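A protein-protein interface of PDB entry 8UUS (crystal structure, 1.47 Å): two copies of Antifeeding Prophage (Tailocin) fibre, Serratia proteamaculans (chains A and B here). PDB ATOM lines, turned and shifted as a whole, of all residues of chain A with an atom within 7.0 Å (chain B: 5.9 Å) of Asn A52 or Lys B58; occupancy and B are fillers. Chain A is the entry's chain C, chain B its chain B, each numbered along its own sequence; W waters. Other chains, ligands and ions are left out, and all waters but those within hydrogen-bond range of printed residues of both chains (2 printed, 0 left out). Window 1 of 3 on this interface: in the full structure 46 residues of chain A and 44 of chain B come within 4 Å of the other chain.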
ATOM      1  N   VAL A  36     -31.417 -21.468  26.474  1.00  0.00           N
ATOM      2  CA  VAL A  36     -31.294 -22.785  25.852  1.00  0.00           C
ATOM      3  C   VAL A  36     -30.340 -23.640  26.675  1.00  0.00           C
ATOM      4  O   VAL A  36     -29.375 -23.144  27.269  1.00  0.00           O
ATOM      5  CB  VAL A  36     -30.859 -22.738  24.370  1.00  0.00           C
ATOM      6  CG1 VAL A  36     -31.871 -21.948  23.545  1.00  0.00           C
ATOM      7  CG2 VAL A  36     -29.465 -22.141  24.229  1.00  0.00           C
ATOM      8  N   GLU A  37     -30.622 -24.938  26.714  1.00  0.00           N
ATOM      9  CA  GLU A  37     -29.778 -25.856  27.464  1.00  0.00           C
ATOM     10  C   GLU A  37     -28.595 -26.274  26.606  1.00  0.00           C
ATOM     11  O   GLU A  37     -28.755 -26.619  25.433  1.00  0.00           O
ATOM     12  CB  GLU A  37     -30.568 -27.087  27.901  1.00  0.00           C
ATOM     13  CG  GLU A  37     -29.690 -28.093  28.644  1.00  0.00           C
ATOM     14  CD  GLU A  37     -30.460 -29.182  29.362  1.00  0.00           C
ATOM     15  OE1 GLU A  37     -31.688 -29.277  29.197  1.00  0.00           O
ATOM     16  OE2 GLU A  37     -29.821 -29.953  30.115  1.00  0.00           O
ATOM     17  N   ALA A  38     -27.408 -26.262  27.223  1.00  0.00           N
ATOM     18  CA  ALA A  38     -26.137 -26.291  26.498  1.00  0.00           C
ATOM     19  C   ALA A  38     -26.086 -27.368  25.415  1.00  0.00           C
ATOM     20  O   ALA A  38     -25.943 -27.066  24.222  1.00  0.00           O
ATOM     21  CB  ALA A  38     -24.994 -26.479  27.497  1.00  0.00           C
ATOM     22  N   SER A  39     -26.195 -28.632  25.812  1.00  0.00           N
ATOM     23  CA  SER A  39     -25.875 -29.757  24.940  1.00  0.00           C
ATOM     24  C   SER A  39     -27.070 -30.264  24.139  1.00  0.00           C
ATOM     25  O   SER A  39     -27.022 -31.387  23.613  1.00  0.00           O
ATOM     26  CB  SER A  39     -25.319 -30.909  25.774  1.00  0.00           C
ATOM     27  OG  SER A  39     -26.257 -31.274  26.769  1.00  0.00           O
ATOM     28  N   LYS A  40     -28.137 -29.475  24.024  1.00  0.00           N
ATOM     29  CA  LYS A  40     -29.394 -29.974  23.487  1.00  0.00           C
ATOM     30  C   LYS A  40     -29.729 -29.403  22.115  1.00  0.00           C
ATOM     31  O   LYS A  40     -30.879 -29.509  21.678  1.00  0.00           O
ATOM     32  CB  LYS A  40     -30.541 -29.745  24.473  1.00  0.00           C
ATOM     33  CG  LYS A  40     -30.310 -30.369  25.840  1.00  0.00           C
ATOM     34  CD  LYS A  40     -30.519 -31.865  25.789  1.00  0.00           C
ATOM     35  CE  LYS A  40     -30.695 -32.448  27.182  1.00  0.00           C
ATOM     36  NZ  LYS A  40     -30.632 -33.930  27.146  1.00  0.00           N
ATOM     37  N   GLY A  41     -28.762 -28.788  21.429  1.00  0.00           N
ATOM     38  CA  GLY A  41     -28.893 -28.544  20.009  1.00  0.00           C
ATOM     39  C   GLY A  41     -29.412 -27.188  19.587  1.00  0.00           C
ATOM     40  O   GLY A  41     -29.506 -26.941  18.380  1.00  0.00           O
ATOM     41  N   LEU A  42     -29.730 -26.300  20.519  1.00  0.00           N
ATOM     42  CA  LEU A  42     -30.309 -25.019  20.149  1.00  0.00           C
ATOM     43  C   LEU A  42     -29.335 -23.888  20.461  1.00  0.00           C
ATOM     44  O   LEU A  42     -28.357 -24.053  21.200  1.00  0.00           O
ATOM     45  CB  LEU A  42     -31.618 -24.791  20.914  1.00  0.00           C
ATOM     46  CG  LEU A  42     -32.775 -25.760  20.651  1.00  0.00           C
ATOM     47  CD1 LEU A  42     -34.055 -25.271  21.338  1.00  0.00           C
ATOM     48  CD2 LEU A  42     -33.038 -26.012  19.178  1.00  0.00           C
ATOM     49  N   GLN A  43     -29.618 -22.728  19.880  1.00  0.00           N
ATOM     50  CA  GLN A  43     -28.879 -21.505  20.134  1.00  0.00           C
ATOM     51  C   GLN A  43     -29.879 -20.362  20.176  1.00  0.00           C
ATOM     52  O   GLN A  43     -31.007 -20.479  19.695  1.00  0.00           O
ATOM     53  CB  GLN A  43     -27.850 -21.214  19.028  1.00  0.00           C
ATOM     54  CG  GLN A  43     -28.464 -21.067  17.634  1.00  0.00           C
ATOM     55  CD  GLN A  43     -27.455 -20.651  16.583  1.00  0.00           C
ATOM     56  OE1 GLN A  43     -26.338 -21.159  16.546  1.00  0.00           O
ATOM     57  NE2 GLN A  43     -27.847 -19.712  15.722  1.00  0.00           N
ATOM     58  N   GLY A  50     -32.819 -20.881  17.337  1.00  0.00           N
ATOM     59  CA  GLY A  50     -32.638 -21.761  16.192  1.00  0.00           C
ATOM     60  C   GLY A  50     -31.844 -22.987  16.581  1.00  0.00           C
ATOM     61  O   GLY A  50     -31.318 -23.081  17.688  1.00  0.00           O
ATOM     62  N   LEU A  51     -31.775 -23.943  15.661  1.00  0.00           N
ATOM     63  CA  LEU A  51     -30.840 -25.048  15.827  1.00  0.00           C
ATOM     64  C   LEU A  51     -29.423 -24.514  15.684  1.00  0.00           C
ATOM     65  O   LEU A  51     -29.173 -23.611  14.881  1.00  0.00           O
ATOM     66  CB  LEU A  51     -31.076 -26.087  14.736  1.00  0.00           C
ATOM     67  CG  LEU A  51     -32.396 -26.847  14.819  1.00  0.00           C
ATOM     68  CD1 LEU A  51     -32.696 -27.593  13.534  1.00  0.00           C
ATOM     69  CD2 LEU A  51     -32.296 -27.807  15.973  1.00  0.00           C
ATOM     70  N   ASN A  52     -28.495 -25.074  16.467  1.00  0.00           N
ATOM     71  CA  ASN A  52     -27.088 -24.747  16.301  1.00  0.00           C
ATOM     72  C   ASN A  52     -26.467 -25.653  15.243  1.00  0.00           C
ATOM     73  O   ASN A  52     -27.135 -26.511  14.656  1.00  0.00           O
ATOM     74  CB  ASN A  52     -26.355 -24.735  17.646  1.00  0.00           C
ATOM     75  CG  ASN A  52     -26.240 -26.117  18.287  1.00  0.00           C
ATOM     76  OD1 ASN A  52     -26.142 -27.143  17.604  1.00  0.00           O
ATOM     77  ND2 ASN A  52     -26.285 -26.147  19.609  1.00  0.00           N
ATOM     78  N   ASN A  53     -25.162 -25.466  14.999  1.00  0.00           N
ATOM     79  CA  ASN A  53     -24.513 -26.141  13.882  1.00  0.00           C
ATOM     80  C   ASN A  53     -24.103 -27.571  14.191  1.00  0.00           C
ATOM     81  O   ASN A  53     -23.615 -28.261  13.285  1.00  0.00           O
ATOM     82  CB  ASN A  53     -23.280 -25.370  13.407  1.00  0.00           C
ATOM     83  CG  ASN A  53     -23.636 -24.121  12.664  1.00  0.00           C
ATOM     84  OD1 ASN A  53     -24.740 -23.994  12.135  1.00  0.00           O
ATOM     85  ND2 ASN A  53     -22.697 -23.183  12.603  1.00  0.00           N
ATOM     86  N   THR A  54     -24.267 -28.026  15.433  1.00  0.00           N
ATOM     87  CA  THR A  54     -23.924 -29.393  15.797  1.00  0.00           C
ATOM     88  C   THR A  54     -25.127 -30.192  16.287  1.00  0.00           C
ATOM     89  O   THR A  54     -24.961 -31.325  16.742  1.00  0.00           O
ATOM     90  CB  THR A  54     -22.793 -29.410  16.825  1.00  0.00           C
ATOM     91  OG1 THR A  54     -23.210 -28.719  18.006  1.00  0.00           O
ATOM     92  CG2 THR A  54     -21.536 -28.747  16.241  1.00  0.00           C
ATOM     93  N   ALA A  55     -26.340 -29.644  16.180  1.00  0.00           N
ATOM     94  CA  ALA A  55     -27.526 -30.406  16.545  1.00  0.00           C
ATOM     95  C   ALA A  55     -27.615 -31.730  15.795  1.00  0.00           C
ATOM     96  O   ALA A  55     -28.195 -32.692  16.310  1.00  0.00           O
ATOM     97  CB  ALA A  55     -28.769 -29.571  16.253  1.00  0.00           C
ATOM     98  N   TRP A  56     -27.069 -31.796  14.576  1.00  0.00           N
ATOM     99  CA  TRP A  56     -27.147 -33.030  13.800  1.00  0.00           C
ATOM    100  C   TRP A  56     -26.460 -34.198  14.503  1.00  0.00           C
ATOM    101  O   TRP A  56     -26.853 -35.347  14.301  1.00  0.00           O
ATOM    102  CB  TRP A  56     -26.577 -32.807  12.394  1.00  0.00           C
ATOM    103  CG  TRP A  56     -25.112 -32.481  12.379  1.00  0.00           C
ATOM    104  CD1 TRP A  56     -24.554 -31.236  12.398  1.00  0.00           C
ATOM    105  CD2 TRP A  56     -24.019 -33.410  12.329  1.00  0.00           C
ATOM    106  NE1 TRP A  56     -23.180 -31.331  12.389  1.00  0.00           N
ATOM    107  CE2 TRP A  56     -22.826 -32.653  12.329  1.00  0.00           C
ATOM    108  CE3 TRP A  56     -23.932 -34.803  12.259  1.00  0.00           C
ATOM    109  CZ2 TRP A  56     -21.557 -33.248  12.275  1.00  0.00           C
ATOM    110  CZ3 TRP A  56     -22.672 -35.391  12.210  1.00  0.00           C
ATOM    111  CH2 TRP A  56     -21.505 -34.615  12.222  1.00  0.00           C
ATOM    112  N   SER B  39     -34.465 -19.808   8.707  1.00  0.00           N
ATOM    113  CA  SER B  39     -33.508 -20.760   8.148  1.00  0.00           C
ATOM    114  C   SER B  39     -32.808 -21.602   9.209  1.00  0.00           C
ATOM    115  O   SER B  39     -31.938 -22.400   8.846  1.00  0.00           O
ATOM    116  CB  SER B  39     -32.431 -20.120   7.258  1.00  0.00           C
ATOM    117  OG  SER B  39     -31.450 -19.492   8.071  1.00  0.00           O
ATOM    118  N   LYS B  40     -33.136 -21.458  10.496  1.00  0.00           N
ATOM    119  CA  LYS B  40     -32.500 -22.259  11.535  1.00  0.00           C
ATOM    120  C   LYS B  40     -33.373 -23.403  12.041  1.00  0.00           C
ATOM    121  O   LYS B  40     -33.058 -23.996  13.083  1.00  0.00           O
ATOM    122  CB  LYS B  40     -32.010 -21.391  12.694  1.00  0.00           C
ATOM    123  CG  LYS B  40     -31.130 -20.235  12.266  1.00  0.00           C
ATOM    124  CD  LYS B  40     -29.827 -20.752  11.692  1.00  0.00           C
ATOM    125  CE  LYS B  40     -28.694 -19.758  11.881  1.00  0.00           C
ATOM    126  NZ  LYS B  40     -27.399 -20.379  11.467  1.00  0.00           N
ATOM    127  N   GLY B  41     -34.458 -23.729  11.343  1.00  0.00           N
ATOM    128  CA  GLY B  41     -35.163 -24.971  11.579  1.00  0.00           C
ATOM    129  C   GLY B  41     -36.304 -24.944  12.579  1.00  0.00           C
ATOM    130  O   GLY B  41     -36.929 -25.984  12.790  1.00  0.00           O
ATOM    131  N   THR B  54     -38.833 -28.682   7.624  1.00  0.00           N
ATOM    132  CA  THR B  54     -37.610 -28.815   6.838  1.00  0.00           C
ATOM    133  C   THR B  54     -36.349 -28.718   7.688  1.00  0.00           C
ATOM    134  O   THR B  54     -35.249 -28.582   7.137  1.00  0.00           O
ATOM    135  CB  THR B  54     -37.565 -27.797   5.692  1.00  0.00           C
ATOM    136  OG1 THR B  54     -37.673 -26.470   6.220  1.00  0.00           O
ATOM    137  CG2 THR B  54     -38.692 -28.053   4.709  1.00  0.00           C
ATOM    138  N   ALA B  55     -36.477 -28.787   9.020  1.00  0.00           N
ATOM    139  CA  ALA B  55     -35.292 -28.815   9.877  1.00  0.00           C
ATOM    140  C   ALA B  55     -34.345 -29.938   9.481  1.00  0.00           C
ATOM    141  O   ALA B  55     -33.124 -29.798   9.614  1.00  0.00           O
ATOM    142  CB  ALA B  55     -35.716 -28.988  11.342  1.00  0.00           C
ATOM    143  N   TRP B  56     -34.892 -31.052   8.990  1.00  0.00           N
ATOM    144  CA  TRP B  56     -34.066 -32.189   8.600  1.00  0.00           C
ATOM    145  C   TRP B  56     -33.073 -31.835   7.497  1.00  0.00           C
ATOM    146  O   TRP B  56     -31.999 -32.442   7.417  1.00  0.00           O
ATOM    147  CB  TRP B  56     -34.960 -33.359   8.182  1.00  0.00           C
ATOM    148  CG  TRP B  56     -35.780 -33.101   6.941  1.00  0.00           C
ATOM    149  CD1 TRP B  56     -37.058 -32.614   6.883  1.00  0.00           C
ATOM    150  CD2 TRP B  56     -35.376 -33.326   5.584  1.00  0.00           C
ATOM    151  NE1 TRP B  56     -37.479 -32.526   5.571  1.00  0.00           N
ATOM    152  CE2 TRP B  56     -36.461 -32.956   4.756  1.00  0.00           C
ATOM    153  CE3 TRP B  56     -34.203 -33.818   4.990  1.00  0.00           C
ATOM    154  CZ2 TRP B  56     -36.404 -33.055   3.362  1.00  0.00           C
ATOM    155  CZ3 TRP B  56     -34.149 -33.911   3.603  1.00  0.00           C
ATOM    156  CH2 TRP B  56     -35.244 -33.530   2.810  1.00  0.00           C
ATOM    157  N   ILE B  57     -33.395 -30.855   6.646  1.00  0.00           N
ATOM    158  CA  ILE B  57     -32.452 -30.447   5.606  1.00  0.00           C
ATOM    159  C   ILE B  57     -31.187 -29.861   6.224  1.00  0.00           C
ATOM    160  O   ILE B  57     -30.067 -30.181   5.810  1.00  0.00           O
ATOM    161  CB  ILE B  57     -33.127 -29.468   4.627  1.00  0.00           C
ATOM    162  CG1 ILE B  57     -34.290 -30.170   3.928  1.00  0.00           C
ATOM    163  CG2 ILE B  57     -32.104 -28.914   3.607  1.00  0.00           C
ATOM    164  CD1 ILE B  57     -35.040 -29.291   2.921  1.00  0.00           C
ATOM    165  N   LYS B  58     -31.347 -28.983   7.218  1.00  0.00           N
ATOM    166  CA  LYS B  58     -30.192 -28.417   7.915  1.00  0.00           C
ATOM    167  C   LYS B  58     -29.380 -29.503   8.609  1.00  0.00           C
ATOM    168  O   LYS B  58     -28.141 -29.455   8.625  1.00  0.00           O
ATOM    169  CB  LYS B  58     -30.669 -27.371   8.932  1.00  0.00           C
ATOM    170  CG  LYS B  58     -29.544 -26.710   9.723  1.00  0.00           C
ATOM    171  CD  LYS B  58     -30.088 -25.580  10.596  1.00  0.00           C
ATOM    172  CE  LYS B  58     -29.065 -25.099  11.606  1.00  0.00           C
ATOM    173  NZ  LYS B  58     -27.913 -24.461  10.912  1.00  0.00           N
ATOM    174  N   MET B  59     -30.064 -30.493   9.183  1.00  0.00           N
ATOM    175  CA  MET B  59     -29.373 -31.599   9.837  1.00  0.00           C
ATOM    176  C   MET B  59     -28.534 -32.400   8.847  1.00  0.00           C
ATOM    177  O   MET B  59     -27.376 -32.732   9.128  1.00  0.00           O
ATOM    178  CB  MET B  59     -30.401 -32.502  10.502  1.00  0.00           C
ATOM    179  CG  MET B  59     -31.215 -31.783  11.545  1.00  0.00           C
ATOM    180  SD  MET B  59     -30.273 -31.214  12.960  1.00  0.00           S
ATOM    181  CE  MET B  59     -31.608 -31.065  14.143  1.00  0.00           C
ATOM    182  N   MET B  60     -29.109 -32.746   7.686  1.00  0.00           N
ATOM    183  CA  MET B  60     -28.374 -33.556   6.714  1.00  0.00           C
ATOM    184  C   MET B  60     -27.235 -32.770   6.074  1.00  0.00           C
ATOM    185  O   MET B  60     -26.188 -33.348   5.740  1.00  0.00           O
ATOM    186  CB  MET B  60     -29.325 -34.057   5.625  1.00  0.00           C
ATOM    187  CG  MET B  60     -30.448 -34.921   6.178  1.00  0.00           C
ATOM    188  SD  MET B  60     -29.871 -36.385   7.058  1.00  0.00           S
ATOM    189  CE  MET B  60     -29.068 -37.268   5.733  1.00  0.00           C
ATOM    190  N   CYS B  61     -27.413 -31.463   5.877  1.00  0.00           N
ATOM    191  CA  CYS B  61     -26.293 -30.653   5.402  1.00  0.00           C
ATOM    192  C   CYS B  61     -25.161 -30.661   6.419  1.00  0.00           C
ATOM    193  O   CYS B  61     -23.984 -30.751   6.053  1.00  0.00           O
ATOM    194  CB  CYS B  61     -26.739 -29.215   5.112  1.00  0.00           C
ATOM    195  SG  CYS B  61     -27.711 -29.020   3.594  1.00  0.00           S
ATOM    196  N   GLY B  62     -25.500 -30.553   7.703  1.00  0.00           N
ATOM    197  CA  GLY B  62     -24.488 -30.668   8.746  1.00  0.00           C
ATOM    198  C   GLY B  62     -23.815 -32.027   8.770  1.00  0.00           C
ATOM    199  O   GLY B  62     -22.593 -32.122   8.892  1.00  0.00           O
ATOM    200  N   LEU B  63     -24.612 -33.097   8.685  1.00  0.00           N
ATOM    201  CA  LEU B  63     -24.080 -34.457   8.695  1.00  0.00           C
ATOM    202  C   LEU B  63     -22.970 -34.637   7.664  1.00  0.00           C
ATOM    203  O   LEU B  63     -21.893 -35.162   7.974  1.00  0.00           O
ATOM    204  CB  LEU B  63     -25.222 -35.436   8.409  1.00  0.00           C
ATOM    205  CG  LEU B  63     -24.861 -36.904   8.146  1.00  0.00           C
ATOM    206  CD1 LEU B  63     -24.158 -37.528   9.355  1.00  0.00           C
ATOM    207  CD2 LEU B  63     -26.076 -37.725   7.718  1.00  0.00           C
ATOM    208  N   PRO B 166     -28.811 -24.291   4.357  1.00  0.00           N
ATOM    209  CA  PRO B 166     -29.438 -23.342   5.289  1.00  0.00           C
ATOM    210  C   PRO B 166     -28.426 -22.723   6.258  1.00  0.00           C
ATOM    211  O   PRO B 166     -27.518 -23.404   6.740  1.00  0.00           O
ATOM    212  CB  PRO B 166     -30.419 -24.205   6.092  1.00  0.00           C
ATOM    213  CG  PRO B 166     -30.505 -25.508   5.419  1.00  0.00           C
ATOM    214  CD  PRO B 166     -29.464 -25.608   4.357  1.00  0.00           C
ATOM    215  OXT PRO B 166     -28.503 -21.540   6.602  1.00  0.00           O
HETATM  216  O   HOH W   1     -26.042 -26.019   9.803  1.00  0.00           O
HETATM  217  O   HOH W   2     -27.058 -22.800  13.141  1.00  0.00           O
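Printed residues of chain B within 4 Å of Leu A51: Lys B40 (2.9 Å), Ala B55 (3.98 Å), Lys B58 (3.6 Å) and Met B59 (3.7 Å). Printed residues of chain B within 4 Å of Asn A52: Lys B58 (3.9 Å). Trp B56 touches none of the printed residues of chain A. Lys B58 touches just these residues of chain A: Leu A51, Asn A52 and Asn A53. Printed residues of chain A within 4 Å of Gly B62: Trp A56. Of the printed residues of chain A, Leu B63 touches Trp A56. The nearest residue of chain B that does not touch Asn A52 is Lys B40 (5.8 Å). The nearest residue of chain A that does not touch Lys B58 is Trp A56 (5.3 Å). The nearest printed residue of chain B that does not touch Leu A51 is Gly B41 (4.1 Å).
Positions printed for both chains: 39, 40, 41, 54, 55 and 56.
The side-chain sulfur (SD) of Met B59 is in hydrogen-bond range of the backbone NH (N) of Trp A56 (3.6 Å). O of Lys B40 sits at hydrogen-bond distance from N of Leu A51 (2.9 Å). The side-chain amide oxygen of Asn A53 is in hydrogen-bond range of the side-chain amino group of Lys B58 (3.4 Å).
Lys B40 touches Gln A43 (CE to NE2, 3.9 Å). Gly A50 touches Lys B40 (CA to CB, 3.6 Å). CD1 of Leu A51 touches CB of Ala B55, at 3.98 Å. O of Leu A51 touches CE of Lys B58, 3.6 Å away. CD1 of Leu A51 touches CE of Met B59, 3.7 Å away. O of Asn A52 touches CE of Lys B58, at 3.9 Å. CB of Ala A55 touches CE of Met B59, 3.8 Å away. O of Gly B62 touches CE2 of Trp A56, at 3.5 Å. Leu B63 touches Trp A56.
Of the 15 printed residues of chain A, 7 touch a printed residue of chain B. Printed residues of chain A that touch a printed residue of chain B: Gln A43, Gly A50, Leu A51, Asn A52, Asn A53, Ala A55 and Trp A56. Hydrophobic or aromatic side chains of chain A within 4 Å of the printed part of chain B: Leu A51, Ala A55 and Trp A56. Among the printed residues, no Asp or Glu carboxylate lies within 4 Å of a Lys or Arg side-chain nitrogen of the other chain.
Water W1 bridges the side-chain amino group (NZ) of Lys B58 and the side-chain amide oxygen (OD1) of Asn A53. Water W2 lies within hydrogen-bond range of OD1 of Asn A53 (2.8 Å), O of Leu A51 (2.9 Å), NZ of Lys B58 (2.9 Å) and NZ of Lys B40 (3.0 Å).
The backbone carbonyl oxygen of Gly A41 lies within hydrogen-bond range of the backbone NH of Asn A52 (2.9 Å). The side-chain amide oxygen (OD1) of Asn A52 lies within hydrogen-bond range of the backbone NH (N) of Ala A55 (2.9 Å). The backbone carbonyl oxygen of Asn A53 lies within hydrogen-bond range of the indole nitrogen of Trp A56, 3.2 Å away. The side-chain amide oxygen of Asn A52 sits at hydrogen-bond distance from the backbone NH of Thr A54, at 3.0 Å. The backbone NH of Gln A43 sits at hydrogen-bond distance from the backbone carbonyl oxygen of Gly A50 (2.8 Å). The side-chain amide nitrogen (ND2) of Asn A52 sits at hydrogen-bond distance from the backbone carbonyl oxygen (O) of Leu A42.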
